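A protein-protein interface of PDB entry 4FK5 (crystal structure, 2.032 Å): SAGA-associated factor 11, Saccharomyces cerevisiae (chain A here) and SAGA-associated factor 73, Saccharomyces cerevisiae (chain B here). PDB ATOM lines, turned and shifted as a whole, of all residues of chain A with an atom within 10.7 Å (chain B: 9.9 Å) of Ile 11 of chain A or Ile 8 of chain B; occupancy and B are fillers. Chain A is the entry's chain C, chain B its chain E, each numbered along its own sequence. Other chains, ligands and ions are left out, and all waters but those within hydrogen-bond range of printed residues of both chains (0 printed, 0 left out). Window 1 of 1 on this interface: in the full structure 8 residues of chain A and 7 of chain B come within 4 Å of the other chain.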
ATOM      1  N   GLU A   4     -25.249 -13.253  18.739  1.00  0.00           N
ATOM      2  CA  GLU A   4     -25.171 -11.865  18.188  1.00  0.00           C
ATOM      3  C   GLU A   4     -24.949 -11.889  16.669  1.00  0.00           C
ATOM      4  O   GLU A   4     -25.605 -11.157  15.937  1.00  0.00           O
ATOM      5  CB  GLU A   4     -24.026 -11.063  18.846  1.00  0.00           C
ATOM      6  CG  GLU A   4     -23.669 -11.476  20.272  1.00  0.00           C
ATOM      7  CD  GLU A   4     -22.780 -12.720  20.335  1.00  0.00           C
ATOM      8  OE1 GLU A   4     -22.582 -13.247  21.451  1.00  0.00           O
ATOM      9  OE2 GLU A   4     -22.289 -13.175  19.270  1.00  0.00           O
ATOM     10  N   THR A   5     -24.009 -12.733  16.216  1.00  0.00           N
ATOM     11  CA  THR A   5     -23.371 -12.562  14.892  1.00  0.00           C
ATOM     12  C   THR A   5     -24.025 -13.446  13.802  1.00  0.00           C
ATOM     13  O   THR A   5     -23.997 -14.670  13.873  1.00  0.00           O
ATOM     14  CB  THR A   5     -21.852 -12.869  14.947  1.00  0.00           C
ATOM     15  OG1 THR A   5     -21.225 -12.060  15.962  1.00  0.00           O
ATOM     16  CG2 THR A   5     -21.195 -12.588  13.579  1.00  0.00           C
ATOM     17  N   ILE A   6     -24.550 -12.804  12.776  1.00  0.00           N
ATOM     18  CA  ILE A   6     -25.388 -13.468  11.798  1.00  0.00           C
ATOM     19  C   ILE A   6     -24.512 -14.091  10.665  1.00  0.00           C
ATOM     20  O   ILE A   6     -23.694 -13.398  10.035  1.00  0.00           O
ATOM     21  CB  ILE A   6     -26.436 -12.479  11.252  1.00  0.00           C
ATOM     22  CG1 ILE A   6     -27.264 -11.906  12.428  1.00  0.00           C
ATOM     23  CG2 ILE A   6     -27.360 -13.176  10.232  1.00  0.00           C
ATOM     24  CD1 ILE A   6     -28.377 -10.959  11.997  1.00  0.00           C
ATOM     25  N   THR A   7     -24.625 -15.410  10.498  1.00  0.00           N
ATOM     26  CA  THR A   7     -23.825 -16.161   9.508  1.00  0.00           C
ATOM     27  C   THR A   7     -24.731 -16.987   8.577  1.00  0.00           C
ATOM     28  O   THR A   7     -25.897 -17.218   8.889  1.00  0.00           O
ATOM     29  CB  THR A   7     -22.857 -17.136  10.202  1.00  0.00           C
ATOM     30  OG1 THR A   7     -23.596 -18.084  10.969  1.00  0.00           O
ATOM     31  CG2 THR A   7     -21.812 -16.365  11.157  1.00  0.00           C
ATOM     32  N   ILE A   8     -24.174 -17.504   7.489  1.00  0.00           N
ATOM     33  CA  ILE A   8     -24.909 -18.435   6.661  1.00  0.00           C
ATOM     34  C   ILE A   8     -25.444 -19.575   7.471  1.00  0.00           C
ATOM     35  O   ILE A   8     -26.617 -20.006   7.277  1.00  0.00           O
ATOM     36  CB  ILE A   8     -24.113 -18.980   5.492  1.00  0.00           C
ATOM     37  CG1 ILE A   8     -23.742 -17.865   4.574  1.00  0.00           C
ATOM     38  CG2 ILE A   8     -24.984 -20.013   4.705  1.00  0.00           C
ATOM     39  CD1 ILE A   8     -23.682 -18.272   3.113  1.00  0.00           C
ATOM     40  N   ASP A   9     -24.646 -20.050   8.424  1.00  0.00           N
ATOM     41  CA  ASP A   9     -25.074 -21.178   9.255  1.00  0.00           C
ATOM     42  C   ASP A   9     -26.216 -20.811  10.217  1.00  0.00           C
ATOM     43  O   ASP A   9     -27.130 -21.614  10.414  1.00  0.00           O
ATOM     44  CB  ASP A   9     -23.903 -21.785  10.026  1.00  0.00           C
ATOM     45  CG  ASP A   9     -23.033 -22.694   9.155  1.00  0.00           C
ATOM     46  OD1 ASP A   9     -23.501 -23.159   8.069  1.00  0.00           O
ATOM     47  OD2 ASP A   9     -21.873 -22.934   9.544  1.00  0.00           O
ATOM     48  N   SER A  10     -26.178 -19.623  10.807  1.00  0.00           N
ATOM     49  CA  SER A  10     -27.227 -19.270  11.770  1.00  0.00           C
ATOM     50  C   SER A  10     -28.566 -19.019  11.059  1.00  0.00           C
ATOM     51  O   SER A  10     -29.615 -19.418  11.551  1.00  0.00           O
ATOM     52  CB  SER A  10     -26.834 -18.081  12.642  1.00  0.00           C
ATOM     53  OG  SER A  10     -26.605 -16.928  11.882  1.00  0.00           O
ATOM     54  N   ILE A  11     -28.509 -18.415   9.898  1.00  0.00           N
ATOM     55  CA  ILE A  11     -29.705 -18.165   9.096  1.00  0.00           C
ATOM     56  C   ILE A  11     -30.276 -19.482   8.606  1.00  0.00           C
ATOM     57  O   ILE A  11     -31.467 -19.738   8.753  1.00  0.00           O
ATOM     58  CB  ILE A  11     -29.412 -17.238   7.877  1.00  0.00           C
ATOM     59  CG1 ILE A  11     -29.019 -15.828   8.326  1.00  0.00           C
ATOM     60  CG2 ILE A  11     -30.645 -17.112   6.987  1.00  0.00           C
ATOM     61  CD1 ILE A  11     -30.109 -15.143   9.127  1.00  0.00           C
ATOM     62  N   SER A  12     -29.409 -20.343   8.064  1.00  0.00           N
ATOM     63  CA  SER A  12     -29.817 -21.714   7.689  1.00  0.00           C
ATOM     64  C   SER A  12     -30.504 -22.472   8.793  1.00  0.00           C
ATOM     65  O   SER A  12     -31.570 -23.095   8.577  1.00  0.00           O
ATOM     66  CB  SER A  12     -28.607 -22.493   7.171  1.00  0.00           C
ATOM     67  OG  SER A  12     -28.137 -21.871   6.003  1.00  0.00           O
ATOM     68  N   ASN A  13     -29.950 -22.416   9.992  1.00  0.00           N
ATOM     69  CA  ASN A  13     -30.583 -22.994  11.133  1.00  0.00           C
ATOM     70  C   ASN A  13     -31.926 -22.338  11.495  1.00  0.00           C
ATOM     71  O   ASN A  13     -32.841 -23.009  11.955  1.00  0.00           O
ATOM     72  CB  ASN A  13     -29.649 -22.936  12.352  1.00  0.00           C
ATOM     73  CG  ASN A  13     -28.682 -24.077  12.381  1.00  0.00           C
ATOM     74  OD1 ASN A  13     -29.040 -25.183  12.734  1.00  0.00           O
ATOM     75  ND2 ASN A  13     -27.450 -23.813  12.019  1.00  0.00           N
ATOM     76  N   GLY A  14     -32.000 -21.019  11.390  1.00  0.00           N
ATOM     77  CA  GLY A  14     -33.311 -20.300  11.568  1.00  0.00           C
ATOM     78  C   GLY A  14     -34.358 -20.823  10.551  1.00  0.00           C
ATOM     79  O   GLY A  14     -35.495 -21.114  10.908  1.00  0.00           O
ATOM     80  N   ILE A  15     -33.949 -20.973   9.306  1.00  0.00           N
ATOM     81  CA  ILE A  15     -34.859 -21.490   8.243  1.00  0.00           C
ATOM     82  C   ILE A  15     -35.356 -22.913   8.547  1.00  0.00           C
ATOM     83  O   ILE A  15     -36.557 -23.166   8.518  1.00  0.00           O
ATOM     84  CB  ILE A  15     -34.233 -21.344   6.822  1.00  0.00           C
ATOM     85  CG1 ILE A  15     -34.148 -19.861   6.465  1.00  0.00           C
ATOM     86  CG2 ILE A  15     -35.047 -22.100   5.747  1.00  0.00           C
ATOM     87  CD1 ILE A  15     -33.177 -19.521   5.357  1.00  0.00           C
ATOM     88  N   LEU A  16     -34.451 -23.797   8.980  1.00  0.00           N
ATOM     89  CA  LEU A  16     -34.814 -25.134   9.337  1.00  0.00           C
ATOM     90  C   LEU A  16     -35.729 -25.144  10.519  1.00  0.00           C
ATOM     91  O   LEU A  16     -36.715 -25.886  10.530  1.00  0.00           O
ATOM     92  CB  LEU A  16     -33.566 -26.001   9.625  1.00  0.00           C
ATOM     93  CG  LEU A  16     -33.826 -27.467   9.932  1.00  0.00           C
ATOM     94  CD1 LEU A  16     -34.634 -28.132   8.845  1.00  0.00           C
ATOM     95  CD2 LEU A  16     -32.523 -28.202  10.175  1.00  0.00           C
ATOM     96  N   ASN A  17     -35.437 -24.293  11.519  1.00  0.00           N
ATOM     97  CA  ASN A  17     -36.277 -24.231  12.686  1.00  0.00           C
ATOM     98  C   ASN A  17     -37.693 -23.727  12.345  1.00  0.00           C
ATOM     99  O   ASN A  17     -38.674 -24.229  12.886  1.00  0.00           O
ATOM    100  CB  ASN A  17     -35.656 -23.379  13.781  1.00  0.00           C
ATOM    101  CG  ASN A  17     -36.458 -23.423  15.103  1.00  0.00           C
ATOM    102  OD1 ASN A  17     -37.137 -22.456  15.443  1.00  0.00           O
ATOM    103  ND2 ASN A  17     -36.378 -24.520  15.826  1.00  0.00           N
ATOM    104  N   ASN A  18     -37.799 -22.777  11.428  1.00  0.00           N
ATOM    105  CA  ASN A  18     -39.130 -22.415  10.909  1.00  0.00           C
ATOM    106  C   ASN A  18     -39.847 -23.632  10.320  1.00  0.00           C
ATOM    107  O   ASN A  18     -40.939 -23.982  10.733  1.00  0.00           O
ATOM    108  CB  ASN A  18     -39.058 -21.207   9.939  1.00  0.00           C
ATOM    109  CG  ASN A  18     -39.003 -19.829  10.689  1.00  0.00           C
ATOM    110  OD1 ASN A  18     -39.455 -18.771  10.162  1.00  0.00           O
ATOM    111  ND2 ASN A  18     -38.407 -19.822  11.817  1.00  0.00           N
ATOM    112  N   LEU A  19     -39.193 -24.341   9.417  1.00  0.00           N
ATOM    113  CA  LEU A  19     -39.835 -25.493   8.804  1.00  0.00           C
ATOM    114  C   LEU A  19     -40.232 -26.539   9.832  1.00  0.00           C
ATOM    115  O   LEU A  19     -41.343 -27.058   9.775  1.00  0.00           O
ATOM    116  CB  LEU A  19     -38.947 -26.109   7.768  1.00  0.00           C
ATOM    117  CG  LEU A  19     -38.693 -25.262   6.524  1.00  0.00           C
ATOM    118  CD1 LEU A  19     -37.410 -25.727   5.838  1.00  0.00           C
ATOM    119  CD2 LEU A  19     -39.889 -25.355   5.555  1.00  0.00           C
ATOM    120  N   ASP B   5     -19.980 -19.695  10.862  1.00  0.00           N
ATOM    121  CA  ASP B   5     -18.831 -19.733   9.910  1.00  0.00           C
ATOM    122  C   ASP B   5     -18.414 -18.276   9.529  1.00  0.00           C
ATOM    123  O   ASP B   5     -18.032 -17.476  10.419  1.00  0.00           O
ATOM    124  CB  ASP B   5     -19.217 -20.586   8.666  1.00  0.00           C
ATOM    125  CG  ASP B   5     -18.047 -21.466   8.142  1.00  0.00           C
ATOM    126  OD1 ASP B   5     -17.203 -21.916   8.956  1.00  0.00           O
ATOM    127  OD2 ASP B   5     -18.016 -21.750   6.922  1.00  0.00           O
ATOM    128  N   ALA B   6     -18.503 -17.932   8.233  1.00  0.00           N
ATOM    129  CA  ALA B   6     -18.312 -16.531   7.772  1.00  0.00           C
ATOM    130  C   ALA B   6     -19.559 -15.669   8.015  1.00  0.00           C
ATOM    131  O   ALA B   6     -20.705 -16.103   7.803  1.00  0.00           O
ATOM    132  CB  ALA B   6     -17.934 -16.494   6.295  1.00  0.00           C
ATOM    133  N   GLU B   7     -19.315 -14.438   8.423  1.00  0.00           N
ATOM    134  CA  GLU B   7     -20.364 -13.507   8.775  1.00  0.00           C
ATOM    135  C   GLU B   7     -20.984 -12.900   7.535  1.00  0.00           C
ATOM    136  O   GLU B   7     -20.290 -12.597   6.572  1.00  0.00           O
ATOM    137  CB  GLU B   7     -19.782 -12.401   9.651  1.00  0.00           C
ATOM    138  CG  GLU B   7     -20.702 -11.209   9.859  1.00  0.00           C
ATOM    139  CD  GLU B   7     -20.111 -10.173  10.817  1.00  0.00           C
ATOM    140  OE1 GLU B   7     -20.146  -8.984  10.480  1.00  0.00           O
ATOM    141  OE2 GLU B   7     -19.632 -10.561  11.911  1.00  0.00           O
ATOM    142  N   ILE B   8     -22.283 -12.659   7.579  1.00  0.00           N
ATOM    143  CA  ILE B   8     -22.996 -12.147   6.399  1.00  0.00           C
ATOM    144  C   ILE B   8     -22.863 -10.642   6.294  1.00  0.00           C
ATOM    145  O   ILE B   8     -23.073  -9.935   7.259  1.00  0.00           O
ATOM    146  CB  ILE B   8     -24.489 -12.546   6.424  1.00  0.00           C
ATOM    147  CG1 ILE B   8     -24.612 -14.079   6.278  1.00  0.00           C
ATOM    148  CG2 ILE B   8     -25.252 -11.837   5.298  1.00  0.00           C
ATOM    149  CD1 ILE B   8     -26.037 -14.635   6.285  1.00  0.00           C
ATOM    150  N   LYS B   9     -22.506 -10.156   5.106  1.00  0.00           N
ATOM    151  CA  LYS B   9     -22.498  -8.735   4.851  1.00  0.00           C
ATOM    152  C   LYS B   9     -23.898  -8.269   4.442  1.00  0.00           C
ATOM    153  O   LYS B   9     -24.423  -7.310   4.985  1.00  0.00           O
ATOM    154  CB  LYS B   9     -21.478  -8.391   3.761  1.00  0.00           C
ATOM    155  CG  LYS B   9     -21.649  -6.990   3.196  1.00  0.00           C
ATOM    156  CD  LYS B   9     -20.497  -6.604   2.278  1.00  0.00           C
ATOM    157  CE  LYS B   9     -20.550  -5.121   1.911  1.00  0.00           C
ATOM    158  NZ  LYS B   9     -19.777  -4.840   0.672  1.00  0.00           N
ATOM    159  N   GLY B  10     -24.495  -8.971   3.487  1.00  0.00           N
ATOM    160  CA  GLY B  10     -25.842  -8.656   3.025  1.00  0.00           C
ATOM    161  C   GLY B  10     -26.240  -9.635   1.933  1.00  0.00           C
ATOM    162  O   GLY B  10     -25.410 -10.478   1.508  1.00  0.00           O
ATOM    163  N   ILE B  11     -27.478  -9.504   1.456  1.00  0.00           N
ATOM    164  CA  ILE B  11     -27.929 -10.182   0.225  1.00  0.00           C
ATOM    165  C   ILE B  11     -27.278  -9.480  -0.977  1.00  0.00           C
ATOM    166  O   ILE B  11     -27.180  -8.254  -1.006  1.00  0.00           O
ATOM    167  CB  ILE B  11     -29.508 -10.162   0.110  1.00  0.00           C
ATOM    168  CG1 ILE B  11     -30.133 -10.878   1.345  1.00  0.00           C
ATOM    169  CG2 ILE B  11     -30.003 -10.827  -1.190  1.00  0.00           C
ATOM    170  CD1 ILE B  11     -31.658 -10.741   1.465  1.00  0.00           C
ATOM    171  N   LYS B  12     -26.776 -10.247  -1.937  1.00  0.00           N
ATOM    172  CA  LYS B  12     -26.278  -9.638  -3.187  1.00  0.00           C
ATOM    173  C   LYS B  12     -27.287  -8.613  -3.756  1.00  0.00           C
ATOM    174  O   LYS B  12     -28.476  -8.919  -3.965  1.00  0.00           O
ATOM    175  CB  LYS B  12     -25.948 -10.699  -4.249  1.00  0.00           C
ATOM    176  CG  LYS B  12     -24.776 -11.614  -3.891  1.00  0.00           C
ATOM    177  CD  LYS B  12     -24.549 -12.663  -4.999  1.00  0.00           C
ATOM    178  CE  LYS B  12     -23.471 -13.679  -4.645  1.00  0.00           C
ATOM    179  NZ  LYS B  12     -22.402 -13.081  -3.787  1.00  0.00           N
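O of Asp 9 of chain A is in hydrogen-bond range of ND2 of Asn 13 of chain A (2.7 Å).
The side-chain hydroxyl (OG) of Ser 10 of chain A sits at hydrogen-bond distance from the backbone NH (N) of Thr 7 of chain A, 2.9 Å away.
The backbone carbonyl oxygen (O) of Ile 8 of chain A lies within hydrogen-bond range of the side-chain hydroxyl (OG) of Ser 12 of chain A.
OG1 of Thr 7 of chain A sits close to N of Asp 9 of chain A.
O of Ile 6 of chain A lies within hydrogen-bond range of N of Ile 8 of chain B (2.9 Å).
Thr 5 of chain A touches Glu 7 of chain B.
Glu 7 of chain B touches Ile 6 of chain A (CA to O, 3.6 Å).
Asp 5 of chain B touches Thr 7 of chain A (N to CG2, 3.8 Å).
Thr 7 of chain A touches Ala 6 of chain B (CB to O, 3.4 Å).
Glu 7 of chain B touches Thr 7 of chain A (CA to CG2, 3.99 Å).
Thr 7 of chain A touches Ile 8 of chain B (C to CD1, 3.5 Å).
Ile 8 of chain A touches Ala 6 of chain B.
CD1 of Ile 8 of chain B touches N of Ile 8 of chain A, at 3.6 Å.
Asp 9 of chain A touches Asp 5 of chain B.
CD1 of Ile 8 of chain B touches CG1 of Ile 11 of chain A (3.8 Å).
Of the 8 printed residues of chain B, 4 touch a printed residue of chain A.
Hydrophobic or aromatic side chains of chain B within 4 Å of the printed part of chain A: Ile 8.
Of the 16 printed residues of chain A, 6 touch a printed residue of chain B.
Among the printed residues, no Asp or Glu carboxylate lies within 4 Å of a Lys or Arg side-chain nitrogen of the other chain.
Printed residues of chain B within 4 Å of Thr 5 of chain A: Glu 7 (3.1 Å).
Printed residues of chain B within 4 Å of Ile 6 of chain A: Glu 7 and Ile 8.
Of the printed residues of chain B, Thr 7 of chain A touches Asp 5 (3.8 Å), Ala 6 (3.4 Å), Glu 7 (3.99 Å) and Ile 8 (3.5 Å).
Of chain B, only Ala 6 (3.8 Å) and Ile 8 (3.6 Å) come within 4 Å of Ile 8 of chain A.
Of the printed residues of chain B, Asp 9 of chain A touches Asp 5.
Of chain B, only Ile 8 (3.8 Å) comes within 4 Å of Ile 11 of chain A.
No residue of chain B comes within 4 Å of Gly 14 of chain A.
Asn 17 of chain A touches none of the printed residues of chain B.
Printed residues of chain A within 4 Å of Asp 5 of chain B: Thr 7 (3.8 Å) and Asp 9 (3.7 Å).
Of the printed residues of chain A, Glu 7 of chain B touches Thr 5 (3.1 Å), Ile 6 (3.6 Å) and Thr 7 (3.99 Å).
Ile 8 of chain B touches just these residues of chain A: Ile 6, Thr 7, Ile 8 and Ile 11.
Lys 9 of chain B touches none of the printed residues of chain A.
The nearest printed residue of chain A that does not touch Asp 5 of chain B is Ile 8 of chain A (5.8 Å).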
